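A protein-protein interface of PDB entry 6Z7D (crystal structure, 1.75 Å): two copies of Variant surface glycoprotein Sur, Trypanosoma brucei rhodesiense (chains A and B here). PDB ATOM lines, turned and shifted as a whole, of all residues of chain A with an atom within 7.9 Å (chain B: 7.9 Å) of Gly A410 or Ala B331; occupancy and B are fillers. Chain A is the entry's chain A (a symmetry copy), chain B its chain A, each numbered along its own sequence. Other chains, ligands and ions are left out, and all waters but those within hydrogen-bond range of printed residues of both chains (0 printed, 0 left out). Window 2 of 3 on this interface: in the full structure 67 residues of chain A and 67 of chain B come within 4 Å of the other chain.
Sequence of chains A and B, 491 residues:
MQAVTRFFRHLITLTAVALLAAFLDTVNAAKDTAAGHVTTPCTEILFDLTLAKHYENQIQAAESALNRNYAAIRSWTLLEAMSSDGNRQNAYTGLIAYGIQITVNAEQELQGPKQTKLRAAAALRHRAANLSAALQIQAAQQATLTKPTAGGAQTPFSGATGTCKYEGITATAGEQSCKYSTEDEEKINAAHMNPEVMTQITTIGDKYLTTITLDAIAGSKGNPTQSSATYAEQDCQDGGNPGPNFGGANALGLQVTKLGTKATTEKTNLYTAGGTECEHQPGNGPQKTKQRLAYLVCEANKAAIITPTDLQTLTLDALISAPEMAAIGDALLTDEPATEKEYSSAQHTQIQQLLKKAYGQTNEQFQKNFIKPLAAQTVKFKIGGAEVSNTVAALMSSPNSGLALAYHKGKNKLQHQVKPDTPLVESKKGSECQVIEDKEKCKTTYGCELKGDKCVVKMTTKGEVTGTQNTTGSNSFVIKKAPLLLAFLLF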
ATOM      1  N   ALA A  81      -0.101 -14.226   3.486  1.00  0.00           N
ATOM      2  CA  ALA A  81      -0.082 -15.296   4.480  1.00  0.00           C
ATOM      3  C   ALA A  81      -1.336 -15.332   5.358  1.00  0.00           C
ATOM      4  O   ALA A  81      -1.635 -16.386   5.935  1.00  0.00           O
ATOM      5  CB  ALA A  81       1.155 -15.163   5.366  1.00  0.00           C
ATOM      6  N   PHE A 381      -1.034 -10.517  17.999  1.00  0.00           N
ATOM      7  CA  PHE A 381      -0.608 -11.878  18.326  1.00  0.00           C
ATOM      8  C   PHE A 381       0.409 -11.816  19.460  1.00  0.00           C
ATOM      9  O   PHE A 381       0.899 -10.745  19.825  1.00  0.00           O
ATOM     10  CB  PHE A 381      -0.006 -12.597  17.115  1.00  0.00           C
ATOM     11  CG  PHE A 381       1.230 -11.934  16.570  1.00  0.00           C
ATOM     12  CD1 PHE A 381       2.489 -12.430  16.866  1.00  0.00           C
ATOM     13  CD2 PHE A 381       1.135 -10.811  15.772  1.00  0.00           C
ATOM     14  CE1 PHE A 381       3.631 -11.812  16.369  1.00  0.00           C
ATOM     15  CE2 PHE A 381       2.277 -10.187  15.276  1.00  0.00           C
ATOM     16  CZ  PHE A 381       3.523 -10.689  15.577  1.00  0.00           C
ATOM     17  N   GLY A 402       9.319  -9.917  10.576  1.00  0.00           N
ATOM     18  CA  GLY A 402       9.540 -11.319  10.267  1.00  0.00           C
ATOM     19  C   GLY A 402       8.713 -12.253  11.129  1.00  0.00           C
ATOM     20  O   GLY A 402       8.176 -13.249  10.642  1.00  0.00           O
ATOM     21  N   LEU A 403       8.602 -11.943  12.419  1.00  0.00           N
ATOM     22  CA  LEU A 403       7.888 -12.813  13.345  1.00  0.00           C
ATOM     23  C   LEU A 403       6.386 -12.834  13.060  1.00  0.00           C
ATOM     24  O   LEU A 403       5.726 -13.872  13.237  1.00  0.00           O
ATOM     25  CB  LEU A 403       8.164 -12.353  14.774  1.00  0.00           C
ATOM     26  CG  LEU A 403       7.448 -13.103  15.884  1.00  0.00           C
ATOM     27  CD1 LEU A 403       7.877 -14.562  15.841  1.00  0.00           C
ATOM     28  CD2 LEU A 403       7.761 -12.469  17.233  1.00  0.00           C
ATOM     29  N   ALA A 404       5.827 -11.698  12.633  1.00  0.00           N
ATOM     30  CA  ALA A 404       4.423 -11.675  12.227  1.00  0.00           C
ATOM     31  C   ALA A 404       4.199 -12.567  11.020  1.00  0.00           C
ATOM     32  O   ALA A 404       3.179 -13.255  10.924  1.00  0.00           O
ATOM     33  CB  ALA A 404       3.971 -10.249  11.910  1.00  0.00           C
ATOM     34  N   LEU A 405       5.149 -12.570  10.087  1.00  0.00           N
ATOM     35  CA  LEU A 405       5.003 -13.411   8.908  1.00  0.00           C
ATOM     36  C   LEU A 405       5.077 -14.883   9.282  1.00  0.00           C
ATOM     37  O   LEU A 405       4.255 -15.697   8.834  1.00  0.00           O
ATOM     38  CB  LEU A 405       6.084 -13.043   7.893  1.00  0.00           C
ATOM     39  CG  LEU A 405       6.192 -13.911   6.648  1.00  0.00           C
ATOM     40  CD1 LEU A 405       4.919 -13.806   5.788  1.00  0.00           C
ATOM     41  CD2 LEU A 405       7.469 -13.562   5.859  1.00  0.00           C
ATOM     42  N   ALA A 406       6.050 -15.242  10.121  1.00  0.00           N
ATOM     43  CA  ALA A 406       6.190 -16.639  10.539  1.00  0.00           C
ATOM     44  C   ALA A 406       4.961 -17.107  11.295  1.00  0.00           C
ATOM     45  O   ALA A 406       4.449 -18.211  11.063  1.00  0.00           O
ATOM     46  CB  ALA A 406       7.442 -16.812  11.409  1.00  0.00           C
ATOM     47  N   TYR A 407       4.471 -16.270  12.204  1.00  0.00           N
ATOM     48  CA  TYR A 407       3.301 -16.627  12.990  1.00  0.00           C
ATOM     49  C   TYR A 407       2.093 -16.907  12.101  1.00  0.00           C
ATOM     50  O   TYR A 407       1.366 -17.879  12.324  1.00  0.00           O
ATOM     51  CB  TYR A 407       3.006 -15.504  13.980  1.00  0.00           C
ATOM     52  CG  TYR A 407       1.769 -15.728  14.804  1.00  0.00           C
ATOM     53  CD1 TYR A 407       1.806 -16.507  15.948  1.00  0.00           C
ATOM     54  CD2 TYR A 407       0.558 -15.159  14.435  1.00  0.00           C
ATOM     55  CE1 TYR A 407       0.678 -16.717  16.702  1.00  0.00           C
ATOM     56  CE2 TYR A 407      -0.589 -15.364  15.186  1.00  0.00           C
ATOM     57  CZ  TYR A 407      -0.529 -16.144  16.326  1.00  0.00           C
ATOM     58  OH  TYR A 407      -1.681 -16.368  17.090  1.00  0.00           O
ATOM     59  N   HIS A 408       1.856 -16.075  11.081  1.00  0.00           N
ATOM     60  CA  HIS A 408       0.635 -16.262  10.295  1.00  0.00           C
ATOM     61  C   HIS A 408       0.797 -17.314   9.209  1.00  0.00           C
ATOM     62  O   HIS A 408      -0.185 -17.973   8.842  1.00  0.00           O
ATOM     63  CB  HIS A 408       0.166 -14.932   9.696  1.00  0.00           C
ATOM     64  CG  HIS A 408      -0.426 -14.021  10.721  1.00  0.00           C
ATOM     65  ND1 HIS A 408       0.291 -12.999  11.306  1.00  0.00           N
ATOM     66  CD2 HIS A 408      -1.633 -14.045  11.340  1.00  0.00           C
ATOM     67  CE1 HIS A 408      -0.466 -12.406  12.212  1.00  0.00           C
ATOM     68  NE2 HIS A 408      -1.641 -13.015  12.246  1.00  0.00           N
ATOM     69  N   LYS A 409       2.015 -17.503   8.696  1.00  0.00           N
ATOM     70  CA  LYS A 409       2.223 -18.576   7.733  1.00  0.00           C
ATOM     71  C   LYS A 409       2.124 -19.942   8.406  1.00  0.00           C
ATOM     72  O   LYS A 409       1.709 -20.916   7.769  1.00  0.00           O
ATOM     73  CB  LYS A 409       3.571 -18.395   7.029  1.00  0.00           C
ATOM     74  CG  LYS A 409       3.726 -19.264   5.775  1.00  0.00           C
ATOM     75  CD  LYS A 409       2.922 -18.741   4.576  1.00  0.00           C
ATOM     76  CE  LYS A 409       3.699 -17.722   3.743  1.00  0.00           C
ATOM     77  NZ  LYS A 409       2.950 -17.369   2.485  1.00  0.00           N
ATOM     78  N   GLY A 410       2.459 -20.021   9.697  1.00  0.00           N
ATOM     79  CA  GLY A 410       2.322 -21.273  10.423  1.00  0.00           C
ATOM     80  C   GLY A 410       0.918 -21.541  10.926  1.00  0.00           C
ATOM     81  O   GLY A 410       0.543 -22.705  11.127  1.00  0.00           O
ATOM     82  N   LYS A 411       0.129 -20.493  11.149  1.00  0.00           N
ATOM     83  CA  LYS A 411      -1.218 -20.681  11.678  1.00  0.00           C
ATOM     84  C   LYS A 411      -2.177 -21.057  10.549  1.00  0.00           C
ATOM     85  O   LYS A 411      -2.184 -20.410   9.494  1.00  0.00           O
ATOM     86  CB  LYS A 411      -1.704 -19.423  12.401  1.00  0.00           C
ATOM     87  CG  LYS A 411      -3.043 -19.612  13.104  1.00  0.00           C
ATOM     88  CD  LYS A 411      -3.785 -18.288  13.290  1.00  0.00           C
ATOM     89  CE  LYS A 411      -3.164 -17.442  14.387  1.00  0.00           C
ATOM     90  NZ  LYS A 411      -3.941 -16.183  14.608  1.00  0.00           N
ATOM     91  N   ASN B  90       7.871 -24.476   4.499  1.00  0.00           N
ATOM     92  CA  ASN B  90       7.985 -23.819   5.800  1.00  0.00           C
ATOM     93  C   ASN B  90       9.430 -23.449   6.093  1.00  0.00           C
ATOM     94  O   ASN B  90       9.697 -22.396   6.678  1.00  0.00           O
ATOM     95  CB  ASN B  90       7.436 -24.702   6.920  1.00  0.00           C
ATOM     96  CG  ASN B  90       5.926 -24.756   6.919  1.00  0.00           C
ATOM     97  OD1 ASN B  90       5.265 -23.945   6.260  1.00  0.00           O
ATOM     98  ND2 ASN B  90       5.368 -25.710   7.653  1.00  0.00           N
ATOM     99  N   THR B  93      10.250 -20.334   4.314  1.00  0.00           N
ATOM    100  CA  THR B  93       9.515 -19.241   4.935  1.00  0.00           C
ATOM    101  C   THR B  93      10.197 -18.784   6.211  1.00  0.00           C
ATOM    102  O   THR B  93      10.200 -17.593   6.530  1.00  0.00           O
ATOM    103  CB  THR B  93       8.080 -19.682   5.224  1.00  0.00           C
ATOM    104  OG1 THR B  93       7.467 -20.121   4.001  1.00  0.00           O
ATOM    105  CG2 THR B  93       7.273 -18.532   5.828  1.00  0.00           C
ATOM    106  N   MET B 325      15.418 -16.930  15.833  1.00  0.00           N
ATOM    107  CA  MET B 325      14.886 -18.166  15.270  1.00  0.00           C
ATOM    108  C   MET B 325      14.107 -19.008  16.275  1.00  0.00           C
ATOM    109  O   MET B 325      13.436 -19.962  15.868  1.00  0.00           O
ATOM    110  CB  MET B 325      16.011 -19.005  14.658  1.00  0.00           C
ATOM    111  CG  MET B 325      16.492 -18.455  13.324  1.00  0.00           C
ATOM    112  SD  MET B 325      15.160 -18.362  12.087  1.00  0.00           S
ATOM    113  CE  MET B 325      14.782 -20.064  11.811  1.00  0.00           C
ATOM    114  N   ALA B 326      14.171 -18.689  17.566  1.00  0.00           N
ATOM    115  CA  ALA B 326      13.375 -19.435  18.537  1.00  0.00           C
ATOM    116  C   ALA B 326      11.893 -19.204  18.300  1.00  0.00           C
ATOM    117  O   ALA B 326      11.151 -20.141  18.012  1.00  0.00           O
ATOM    118  CB  ALA B 326      13.766 -19.043  19.961  1.00  0.00           C
ATOM    119  N   ALA B 327      11.456 -17.938  18.354  1.00  0.00           N
ATOM    120  CA  ALA B 327      10.047 -17.627  18.119  1.00  0.00           C
ATOM    121  C   ALA B 327       9.626 -17.915  16.678  1.00  0.00           C
ATOM    122  O   ALA B 327       8.480 -18.294  16.434  1.00  0.00           O
ATOM    123  CB  ALA B 327       9.774 -16.163  18.472  1.00  0.00           C
ATOM    124  N   ILE B 328      10.522 -17.735  15.705  1.00  0.00           N
ATOM    125  CA  ILE B 328      10.161 -18.038  14.323  1.00  0.00           C
ATOM    126  C   ILE B 328       9.977 -19.536  14.150  1.00  0.00           C
ATOM    127  O   ILE B 328       8.930 -19.999  13.678  1.00  0.00           O
ATOM    128  CB  ILE B 328      11.214 -17.457  13.355  1.00  0.00           C
ATOM    129  CG1 ILE B 328      11.050 -15.930  13.276  1.00  0.00           C
ATOM    130  CG2 ILE B 328      11.145 -18.150  11.976  1.00  0.00           C
ATOM    131  CD1 ILE B 328      12.209 -15.218  12.613  1.00  0.00           C
ATOM    132  N   GLY B 329      10.957 -20.324  14.600  1.00  0.00           N
ATOM    133  CA  GLY B 329      10.834 -21.772  14.496  1.00  0.00           C
ATOM    134  C   GLY B 329       9.665 -22.327  15.294  1.00  0.00           C
ATOM    135  O   GLY B 329       8.978 -23.260  14.856  1.00  0.00           O
ATOM    136  N   ASP B 330       9.422 -21.766  16.477  1.00  0.00           N
ATOM    137  CA  ASP B 330       8.264 -22.185  17.254  1.00  0.00           C
ATOM    138  C   ASP B 330       6.969 -21.899  16.506  1.00  0.00           C
ATOM    139  O   ASP B 330       5.985 -22.629  16.663  1.00  0.00           O
ATOM    140  CB  ASP B 330       8.268 -21.483  18.612  1.00  0.00           C
ATOM    141  CG  ASP B 330       7.035 -21.819  19.444  1.00  0.00           C
ATOM    142  OD1 ASP B 330       6.768 -23.022  19.669  1.00  0.00           O
ATOM    143  OD2 ASP B 330       6.334 -20.877  19.875  1.00  0.00           O
ATOM    144  N   ALA B 331       6.951 -20.844  15.690  1.00  0.00           N
ATOM    145  CA  ALA B 331       5.752 -20.454  14.956  1.00  0.00           C
ATOM    146  C   ALA B 331       5.534 -21.315  13.723  1.00  0.00           C
ATOM    147  O   ALA B 331       4.387 -21.542  13.322  1.00  0.00           O
ATOM    148  CB  ALA B 331       5.865 -18.970  14.552  1.00  0.00           C
ATOM    149  N   LEU B 332       6.612 -21.834  13.131  1.00  0.00           N
ATOM    150  CA  LEU B 332       6.547 -22.538  11.859  1.00  0.00           C
ATOM    151  C   LEU B 332       6.728 -24.045  11.952  1.00  0.00           C
ATOM    152  O   LEU B 332       6.404 -24.740  10.979  1.00  0.00           O
ATOM    153  CB  LEU B 332       7.621 -22.005  10.899  1.00  0.00           C
ATOM    154  CG  LEU B 332       7.282 -20.730  10.142  1.00  0.00           C
ATOM    155  CD1 LEU B 332       8.561 -19.973   9.777  1.00  0.00           C
ATOM    156  CD2 LEU B 332       6.444 -21.045   8.907  1.00  0.00           C
ATOM    157  N   LEU B 333       7.262 -24.561  13.063  1.00  0.00           N
ATOM    158  CA  LEU B 333       7.640 -25.982  13.134  1.00  0.00           C
ATOM    159  C   LEU B 333       6.845 -26.858  14.137  1.00  0.00           C
ATOM    160  O   LEU B 333       6.621 -26.507  15.301  1.00  0.00           O
ATOM    161  CB  LEU B 333       9.139 -26.067  13.437  1.00  0.00           C
ATOM    162  CG  LEU B 333       9.993 -25.181  12.527  1.00  0.00           C
ATOM    163  CD1 LEU B 333      11.481 -25.242  12.878  1.00  0.00           C
ATOM    164  CD2 LEU B 333       9.775 -25.563  11.077  1.00  0.00           C
ATOM    165  N   ILE B 351      13.272 -26.373  20.680  1.00  0.00           N
ATOM    166  CA  ILE B 351      13.149 -25.614  19.425  1.00  0.00           C
ATOM    167  C   ILE B 351      14.315 -25.881  18.491  1.00  0.00           C
ATOM    168  O   ILE B 351      14.124 -26.103  17.295  1.00  0.00           O
ATOM    169  CB  ILE B 351      13.038 -24.113  19.667  1.00  0.00           C
ATOM    170  CG1 ILE B 351      11.752 -23.773  20.408  1.00  0.00           C
ATOM    171  CG2 ILE B 351      13.061 -23.360  18.328  1.00  0.00           C
ATOM    172  CD1 ILE B 351      10.532 -24.190  19.664  1.00  0.00           C
ATOM    173  N   LEU B 354      13.893 -28.963  16.588  1.00  0.00           N
ATOM    174  CA  LEU B 354      13.034 -28.705  15.434  1.00  0.00           C
ATOM    175  C   LEU B 354      13.784 -27.984  14.314  1.00  0.00           C
ATOM    176  O   LEU B 354      13.558 -28.265  13.127  1.00  0.00           O
ATOM    177  CB  LEU B 354      11.811 -27.889  15.854  1.00  0.00           C
ATOM    178  CG  LEU B 354      10.867 -28.605  16.821  1.00  0.00           C
ATOM    179  CD1 LEU B 354       9.648 -27.747  17.091  1.00  0.00           C
ATOM    180  CD2 LEU B 354      10.467 -29.971  16.286  1.00  0.00           C
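No position is printed for both chains. Of the 7 pairs that touch across the chains among the printed residues, none has its exchanged pair printed and touching as well.
Of chain B, only Ala B331 (3.6 Å) comes within 4 Å of Gly A410. Ala B331 touches just these residues of chain A: Ala A406 (3.8 Å), Tyr A407 (3.8 Å) and Gly A410 (3.6 Å). Printed residues of chain B within 4 Å of Tyr A407: Ala B331. Printed residues of chain A within 4 Å of Thr B93: Lys A409. Printed residues of chain A within 4 Å of Leu B332: Ala A406. Ala A81 touches none of the printed residues of chain B. Met B325 touches none of the printed residues of chain A. The nearest residue of chain B that does not touch Gly A410 is Leu B332 (4.2 Å). The nearest residue of chain A that does not touch Ala B331 is Lys A411 (4.9 Å).
The side-chain amino group of Lys A411 lies close to the side-chain hydroxyl of Tyr A407, at 3.4 Å.
Of the 12 printed residues of chain A, 5 touch a printed residue of chain B. Hydrophobic or aromatic side chains of chain A that line the printed part of chain B: Leu A403 and Ala A406. Among the printed residues, 7 pairs touch across the chains. Among the printed residues, no Asp or Glu carboxylate lies within 4 Å of a Lys or Arg side-chain nitrogen of the other chain.
Among the printed residues, pairs that only touch across the chains: Leu A403 with Ala B327 (3.6 Å), Ala A406 with Ile B328 (3.98 Å), Ala A406 with Ala B331 (3.8 Å), Ala A406 with Leu B332 (3.7 Å), Tyr A407 with Ala B331 (3.8 Å), Lys A409 with Thr B93 (3.6 Å) and Gly A410 with Ala B331 (3.6 Å).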
